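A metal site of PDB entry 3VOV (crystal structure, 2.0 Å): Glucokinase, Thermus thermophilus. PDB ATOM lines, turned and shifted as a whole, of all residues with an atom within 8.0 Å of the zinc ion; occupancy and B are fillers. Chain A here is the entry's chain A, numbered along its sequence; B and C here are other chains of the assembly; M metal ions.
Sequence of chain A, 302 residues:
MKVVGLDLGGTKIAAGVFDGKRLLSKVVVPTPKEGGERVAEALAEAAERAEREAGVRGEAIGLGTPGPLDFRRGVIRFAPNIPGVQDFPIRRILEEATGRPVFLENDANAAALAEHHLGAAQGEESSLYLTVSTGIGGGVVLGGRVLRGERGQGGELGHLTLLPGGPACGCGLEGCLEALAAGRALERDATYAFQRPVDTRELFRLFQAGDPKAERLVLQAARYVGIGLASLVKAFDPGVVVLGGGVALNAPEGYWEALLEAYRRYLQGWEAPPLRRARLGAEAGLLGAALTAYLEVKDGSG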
ATOM      1  N   ILE A 136      -3.518   2.806  19.789  1.00  0.00           N
ATOM      2  CA  ILE A 136      -4.558   3.148  20.744  1.00  0.00           C
ATOM      3  C   ILE A 136      -4.953   4.568  20.507  1.00  0.00           C
ATOM      4  O   ILE A 136      -4.109   5.469  20.473  1.00  0.00           O
ATOM      5  CB  ILE A 136      -4.137   2.890  22.214  1.00  0.00           C
ATOM      6  CG1 ILE A 136      -4.103   1.391  22.474  1.00  0.00           C
ATOM      7  CG2 ILE A 136      -5.153   3.552  23.229  1.00  0.00           C
ATOM      8  CD1 ILE A 136      -3.766   1.063  23.948  1.00  0.00           C
ATOM      9  N   GLU A 156      -6.008  12.712  22.592  1.00  0.00           N
ATOM     10  CA  GLU A 156      -4.940  11.803  22.125  1.00  0.00           C
ATOM     11  C   GLU A 156      -4.627  10.837  23.239  1.00  0.00           C
ATOM     12  O   GLU A 156      -3.523  10.811  23.790  1.00  0.00           O
ATOM     13  CB  GLU A 156      -3.691  12.594  21.661  1.00  0.00           C
ATOM     14  CG  GLU A 156      -3.837  13.104  20.211  1.00  0.00           C
ATOM     15  CD  GLU A 156      -3.774  11.968  19.149  1.00  0.00           C
ATOM     16  OE1 GLU A 156      -3.402  10.814  19.435  1.00  0.00           O
ATOM     17  OE2 GLU A 156      -4.092  12.254  17.998  1.00  0.00           O
ATOM     18  N   GLY A 158      -4.191   7.693  23.714  1.00  0.00           N
ATOM     19  CA  GLY A 158      -3.182   6.637  23.672  1.00  0.00           C
ATOM     20  C   GLY A 158      -1.804   7.170  24.020  1.00  0.00           C
ATOM     21  O   GLY A 158      -0.869   6.367  24.156  1.00  0.00           O
ATOM     22  N   HIS A 159      -1.647   8.498  24.141  1.00  0.00           N
ATOM     23  CA  HIS A 159      -0.321   9.038  24.405  1.00  0.00           C
ATOM     24  C   HIS A 159      -0.139   9.668  25.767  1.00  0.00           C
ATOM     25  O   HIS A 159       0.828  10.393  25.986  1.00  0.00           O
ATOM     26  CB  HIS A 159       0.226   9.871  23.232  1.00  0.00           C
ATOM     27  CG  HIS A 159       0.221   9.102  21.941  1.00  0.00           C
ATOM     28  ND1 HIS A 159       1.176   8.165  21.640  1.00  0.00           N
ATOM     29  CD2 HIS A 159      -0.711   9.019  20.961  1.00  0.00           C
ATOM     30  CE1 HIS A 159       0.885   7.585  20.486  1.00  0.00           C
ATOM     31  NE2 HIS A 159      -0.279   8.077  20.069  1.00  0.00           N
ATOM     32  N   LEU A 160      -1.050   9.381  26.691  1.00  0.00           N
ATOM     33  CA  LEU A 160      -0.746   9.696  28.106  1.00  0.00           C
ATOM     34  C   LEU A 160       0.384   8.779  28.584  1.00  0.00           C
ATOM     35  O   LEU A 160       0.393   7.593  28.278  1.00  0.00           O
ATOM     36  CB  LEU A 160      -1.994   9.540  28.993  1.00  0.00           C
ATOM     37  CG  LEU A 160      -2.702  10.942  28.909  1.00  0.00           C
ATOM     38  CD1 LEU A 160      -3.794  10.930  27.808  1.00  0.00           C
ATOM     39  CD2 LEU A 160      -3.274  11.466  30.223  1.00  0.00           C
ATOM     40  N   THR A 161       1.321   9.350  29.330  1.00  0.00           N
ATOM     41  CA  THR A 161       2.470   8.627  29.832  1.00  0.00           C
ATOM     42  C   THR A 161       2.057   7.808  31.067  1.00  0.00           C
ATOM     43  O   THR A 161       1.679   8.395  32.068  1.00  0.00           O
ATOM     44  CB  THR A 161       3.568   9.631  30.264  1.00  0.00           C
ATOM     45  OG1 THR A 161       3.938  10.432  29.136  1.00  0.00           O
ATOM     46  CG2 THR A 161       4.820   8.898  30.844  1.00  0.00           C
ATOM     47  N   PRO A 167       8.622   1.454  27.115  1.00  0.00           N
ATOM     48  CA  PRO A 167       9.067   1.254  25.735  1.00  0.00           C
ATOM     49  C   PRO A 167       8.819   2.422  24.801  1.00  0.00           C
ATOM     50  O   PRO A 167       7.823   3.132  24.986  1.00  0.00           O
ATOM     51  CB  PRO A 167       8.283   0.038  25.262  1.00  0.00           C
ATOM     52  CG  PRO A 167       7.674  -0.575  26.468  1.00  0.00           C
ATOM     53  CD  PRO A 167       7.507   0.553  27.468  1.00  0.00           C
ATOM     54  N   ALA A 168       9.738   2.628  23.844  1.00  0.00           N
ATOM     55  CA  ALA A 168       9.637   3.695  22.859  1.00  0.00           C
ATOM     56  C   ALA A 168       8.291   3.662  22.187  1.00  0.00           C
ATOM     57  O   ALA A 168       7.786   2.549  21.843  1.00  0.00           O
ATOM     58  CB  ALA A 168      10.759   3.558  21.816  1.00  0.00           C
ATOM     59  N   CYS A 169       7.675   4.851  22.049  1.00  0.00           N
ATOM     60  CA  CYS A 169       6.420   5.026  21.329  1.00  0.00           C
ATOM     61  C   CYS A 169       6.664   5.594  19.929  1.00  0.00           C
ATOM     62  O   CYS A 169       7.623   6.325  19.700  1.00  0.00           O
ATOM     63  CB  CYS A 169       5.496   6.018  22.073  1.00  0.00           C
ATOM     64  SG  CYS A 169       3.772   6.014  21.398  1.00  0.00           S
ATOM     65  N   GLY A 170       5.774   5.257  19.000  1.00  0.00           N
ATOM     66  CA  GLY A 170       5.757   5.835  17.651  1.00  0.00           C
ATOM     67  C   GLY A 170       5.665   7.359  17.677  1.00  0.00           C
ATOM     68  O   GLY A 170       6.125   8.014  16.738  1.00  0.00           O
ATOM     69  N   CYS A 171       5.100   7.933  18.744  1.00  0.00           N
ATOM     70  CA  CYS A 171       4.892   9.397  18.749  1.00  0.00           C
ATOM     71  C   CYS A 171       6.169  10.177  19.024  1.00  0.00           C
ATOM     72  O   CYS A 171       6.237  11.362  18.715  1.00  0.00           O
ATOM     73  CB  CYS A 171       3.778   9.837  19.699  1.00  0.00           C
ATOM     74  SG  CYS A 171       4.319   9.758  21.459  1.00  0.00           S
ATOM     75  N   GLY A 172       7.164   9.512  19.593  1.00  0.00           N
ATOM     76  CA  GLY A 172       8.434  10.154  19.911  1.00  0.00           C
ATOM     77  C   GLY A 172       8.691  10.117  21.424  1.00  0.00           C
ATOM     78  O   GLY A 172       9.790  10.475  21.862  1.00  0.00           O
ATOM     79  N   LEU A 173       7.703   9.688  22.208  1.00  0.00           N
ATOM     80  CA  LEU A 173       7.911   9.521  23.667  1.00  0.00           C
ATOM     81  C   LEU A 173       8.210   8.034  24.022  1.00  0.00           C
ATOM     82  O   LEU A 173       8.636   7.270  23.166  1.00  0.00           O
ATOM     83  CB  LEU A 173       6.703  10.036  24.473  1.00  0.00           C
ATOM     84  CG  LEU A 173       6.201  11.395  24.026  1.00  0.00           C
ATOM     85  CD1 LEU A 173       4.926  11.841  24.864  1.00  0.00           C
ATOM     86  CD2 LEU A 173       7.331  12.397  24.076  1.00  0.00           C
ATOM     87  N   GLU A 174       7.947   7.648  25.275  1.00  0.00           N
ATOM     88  CA  GLU A 174       8.117   6.262  25.730  1.00  0.00           C
ATOM     89  C   GLU A 174       7.129   6.048  26.876  1.00  0.00           C
ATOM     90  O   GLU A 174       6.782   7.020  27.567  1.00  0.00           O
ATOM     91  CB  GLU A 174       9.585   5.980  26.181  1.00  0.00           C
ATOM     92  CG  GLU A 174       9.945   6.196  27.694  1.00  0.00           C
ATOM     93  CD  GLU A 174       9.823   7.631  28.216  1.00  0.00           C
ATOM     94  OE1 GLU A 174       9.966   8.610  27.439  1.00  0.00           O
ATOM     95  OE2 GLU A 174       9.705   7.801  29.453  1.00  0.00           O
ATOM     96  N   GLY A 175       6.631   4.829  27.022  1.00  0.00           N
ATOM     97  CA  GLY A 175       5.739   4.495  28.161  1.00  0.00           C
ATOM     98  C   GLY A 175       4.316   5.044  27.955  1.00  0.00           C
ATOM     99  O   GLY A 175       3.553   5.121  28.919  1.00  0.00           O
ATOM    100  N   CYS A 176       3.984   5.462  26.725  1.00  0.00           N
ATOM    101  CA  CYS A 176       2.617   5.858  26.371  1.00  0.00           C
ATOM    102  C   CYS A 176       1.740   4.639  26.510  1.00  0.00           C
ATOM    103  O   CYS A 176       2.187   3.522  26.246  1.00  0.00           O
ATOM    104  CB  CYS A 176       2.557   6.287  24.895  1.00  0.00           C
ATOM    105  SG  CYS A 176       3.347   7.853  24.637  1.00  0.00           S
ATOM    106  N   LEU A 177       0.494   4.851  26.893  1.00  0.00           N
ATOM    107  CA  LEU A 177      -0.525   3.781  26.827  1.00  0.00           C
ATOM    108  C   LEU A 177      -0.465   2.984  25.501  1.00  0.00           C
ATOM    109  O   LEU A 177      -0.467   1.751  25.518  1.00  0.00           O
ATOM    110  CB  LEU A 177      -1.922   4.401  26.985  1.00  0.00           C
ATOM    111  CG  LEU A 177      -3.110   3.452  26.950  1.00  0.00           C
ATOM    112  CD1 LEU A 177      -2.944   2.238  27.837  1.00  0.00           C
ATOM    113  CD2 LEU A 177      -4.395   4.257  27.399  1.00  0.00           C
ATOM    114  N   GLU A 178      -0.425   3.687  24.358  1.00  0.00           N
ATOM    115  CA  GLU A 178      -0.310   2.952  23.072  1.00  0.00           C
ATOM    116  C   GLU A 178       0.944   2.038  23.005  1.00  0.00           C
ATOM    117  O   GLU A 178       0.868   0.853  22.606  1.00  0.00           O
ATOM    118  CB  GLU A 178      -0.340   3.921  21.885  1.00  0.00           C
ATOM    119  CG  GLU A 178       0.093   3.328  20.527  1.00  0.00           C
ATOM    120  CD  GLU A 178      -0.171   4.280  19.357  1.00  0.00           C
ATOM    121  OE1 GLU A 178      -1.354   4.460  18.973  1.00  0.00           O
ATOM    122  OE2 GLU A 178       0.792   4.813  18.802  1.00  0.00           O
ATOM    123  N   ALA A 179       2.084   2.589  23.426  1.00  0.00           N
ATOM    124  CA  ALA A 179       3.364   1.840  23.444  1.00  0.00           C
ATOM    125  C   ALA A 179       3.349   0.651  24.394  1.00  0.00           C
ATOM    126  O   ALA A 179       4.136  -0.302  24.253  1.00  0.00           O
ATOM    127  CB  ALA A 179       4.529   2.788  23.816  1.00  0.00           C
ATOM    128  N   LEU A 180       2.442   0.678  25.366  1.00  0.00           N
ATOM    129  CA  LEU A 180       2.328  -0.456  26.300  1.00  0.00           C
ATOM    130  C   LEU A 180       1.299  -1.522  25.929  1.00  0.00           C
ATOM    131  O   LEU A 180       1.462  -2.687  26.299  1.00  0.00           O
ATOM    132  CB  LEU A 180       2.003   0.043  27.715  1.00  0.00           C
ATOM    133  CG  LEU A 180       2.976   0.978  28.395  1.00  0.00           C
ATOM    134  CD1 LEU A 180       2.307   1.715  29.558  1.00  0.00           C
ATOM    135  CD2 LEU A 180       4.219   0.157  28.829  1.00  0.00           C
ATOM    136  N   LYS B 234      -1.857  15.955  26.172  1.00  0.00           N
ATOM    137  CA  LYS B 234      -2.357  14.979  25.184  1.00  0.00           C
ATOM    138  C   LYS B 234      -3.877  14.785  25.373  1.00  0.00           C
ATOM    139  O   LYS B 234      -4.609  14.500  24.431  1.00  0.00           O
ATOM    140  CB  LYS B 234      -1.685  13.599  25.383  1.00  0.00           C
ATOM    141  CG  LYS B 234      -0.154  13.610  25.551  1.00  0.00           C
ATOM    142  CD  LYS B 234       0.547  14.175  24.362  1.00  0.00           C
ATOM    143  CE  LYS B 234       2.062  13.905  24.476  1.00  0.00           C
ATOM    144  NZ  LYS B 234       2.686  14.256  25.807  1.00  0.00           N
ATOM    145  N   GLN B 268       8.249  16.132  22.823  1.00  0.00           N
ATOM    146  CA  GLN B 268       8.949  15.724  21.574  1.00  0.00           C
ATOM    147  C   GLN B 268       7.955  14.940  20.714  1.00  0.00           C
ATOM    148  O   GLN B 268       7.403  13.910  21.149  1.00  0.00           O
ATOM    149  CB  GLN B 268      10.173  14.847  21.856  1.00  0.00           C
ATOM    150  CG  GLN B 268      11.318  15.620  22.484  1.00  0.00           C
ATOM    151  CD  GLN B 268      12.505  14.754  22.983  1.00  0.00           C
ATOM    152  OE1 GLN B 268      13.344  15.285  23.718  1.00  0.00           O
ATOM    153  NE2 GLN B 268      12.562  13.444  22.621  1.00  0.00           N
ATOM    154  N   TRP B 270       5.299  16.545  19.442  1.00  0.00           N
ATOM    155  CA  TRP B 270       4.014  17.209  19.736  1.00  0.00           C
ATOM    156  C   TRP B 270       4.152  18.723  19.666  1.00  0.00           C
ATOM    157  O   TRP B 270       5.256  19.232  19.762  1.00  0.00           O
ATOM    158  CB  TRP B 270       3.532  16.792  21.148  1.00  0.00           C
ATOM    159  CG  TRP B 270       3.271  15.332  21.242  1.00  0.00           C
ATOM    160  CD1 TRP B 270       4.202  14.340  21.480  1.00  0.00           C
ATOM    161  CD2 TRP B 270       2.014  14.676  21.066  1.00  0.00           C
ATOM    162  NE1 TRP B 270       3.578  13.115  21.439  1.00  0.00           N
ATOM    163  CE2 TRP B 270       2.238  13.294  21.206  1.00  0.00           C
ATOM    164  CE3 TRP B 270       0.715  15.133  20.769  1.00  0.00           C
ATOM    165  CZ2 TRP B 270       1.207  12.343  21.065  1.00  0.00           C
ATOM    166  CZ3 TRP B 270      -0.325  14.181  20.664  1.00  0.00           C
ATOM    167  CH2 TRP B 270      -0.055  12.808  20.808  1.00  0.00           C
ATOM    168  N   TYR C 192       9.568  -1.008  16.411  1.00  0.00           N
ATOM    169  CA  TYR C 192       8.225  -0.554  16.819  1.00  0.00           C
ATOM    170  C   TYR C 192       8.014   0.935  16.566  1.00  0.00           C
ATOM    171  O   TYR C 192       7.026   1.331  15.922  1.00  0.00           O
ATOM    172  CB  TYR C 192       7.946  -0.888  18.292  1.00  0.00           C
ATOM    173  CG  TYR C 192       6.566  -0.369  18.716  1.00  0.00           C
ATOM    174  CD1 TYR C 192       5.399  -1.014  18.287  1.00  0.00           C
ATOM    175  CD2 TYR C 192       6.447   0.792  19.494  1.00  0.00           C
ATOM    176  CE1 TYR C 192       4.113  -0.517  18.653  1.00  0.00           C
ATOM    177  CE2 TYR C 192       5.190   1.275  19.876  1.00  0.00           C
ATOM    178  CZ  TYR C 192       4.039   0.633  19.452  1.00  0.00           C
ATOM    179  OH  TYR C 192       2.822   1.148  19.845  1.00  0.00           O
HETATM  180 ZN    ZN M   1       3.120   7.990  22.351  1.00  0.00          ZN
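Of the 24 residues printed, 4 come within 4 Å of the zinc ion.
The side-chain sulfur (SG) of Cys 171 lies close to the backbone NH (N) of Leu 173 (3.5 Å). The side-chain sulfur of Cys 171 lies close to the indole nitrogen of Trp 270 of chain B, 3.4 Å away.
The zinc ion is bound by a ring nitrogen (ND1) of His 159 (2.1 Å), the side-chain sulfur (SG) of Cys 169 (2.3 Å), the side-chain sulfur (SG) of Cys 176 (2.3 Å) and the side-chain sulfur (SG) of Cys 171 (2.3 Å).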
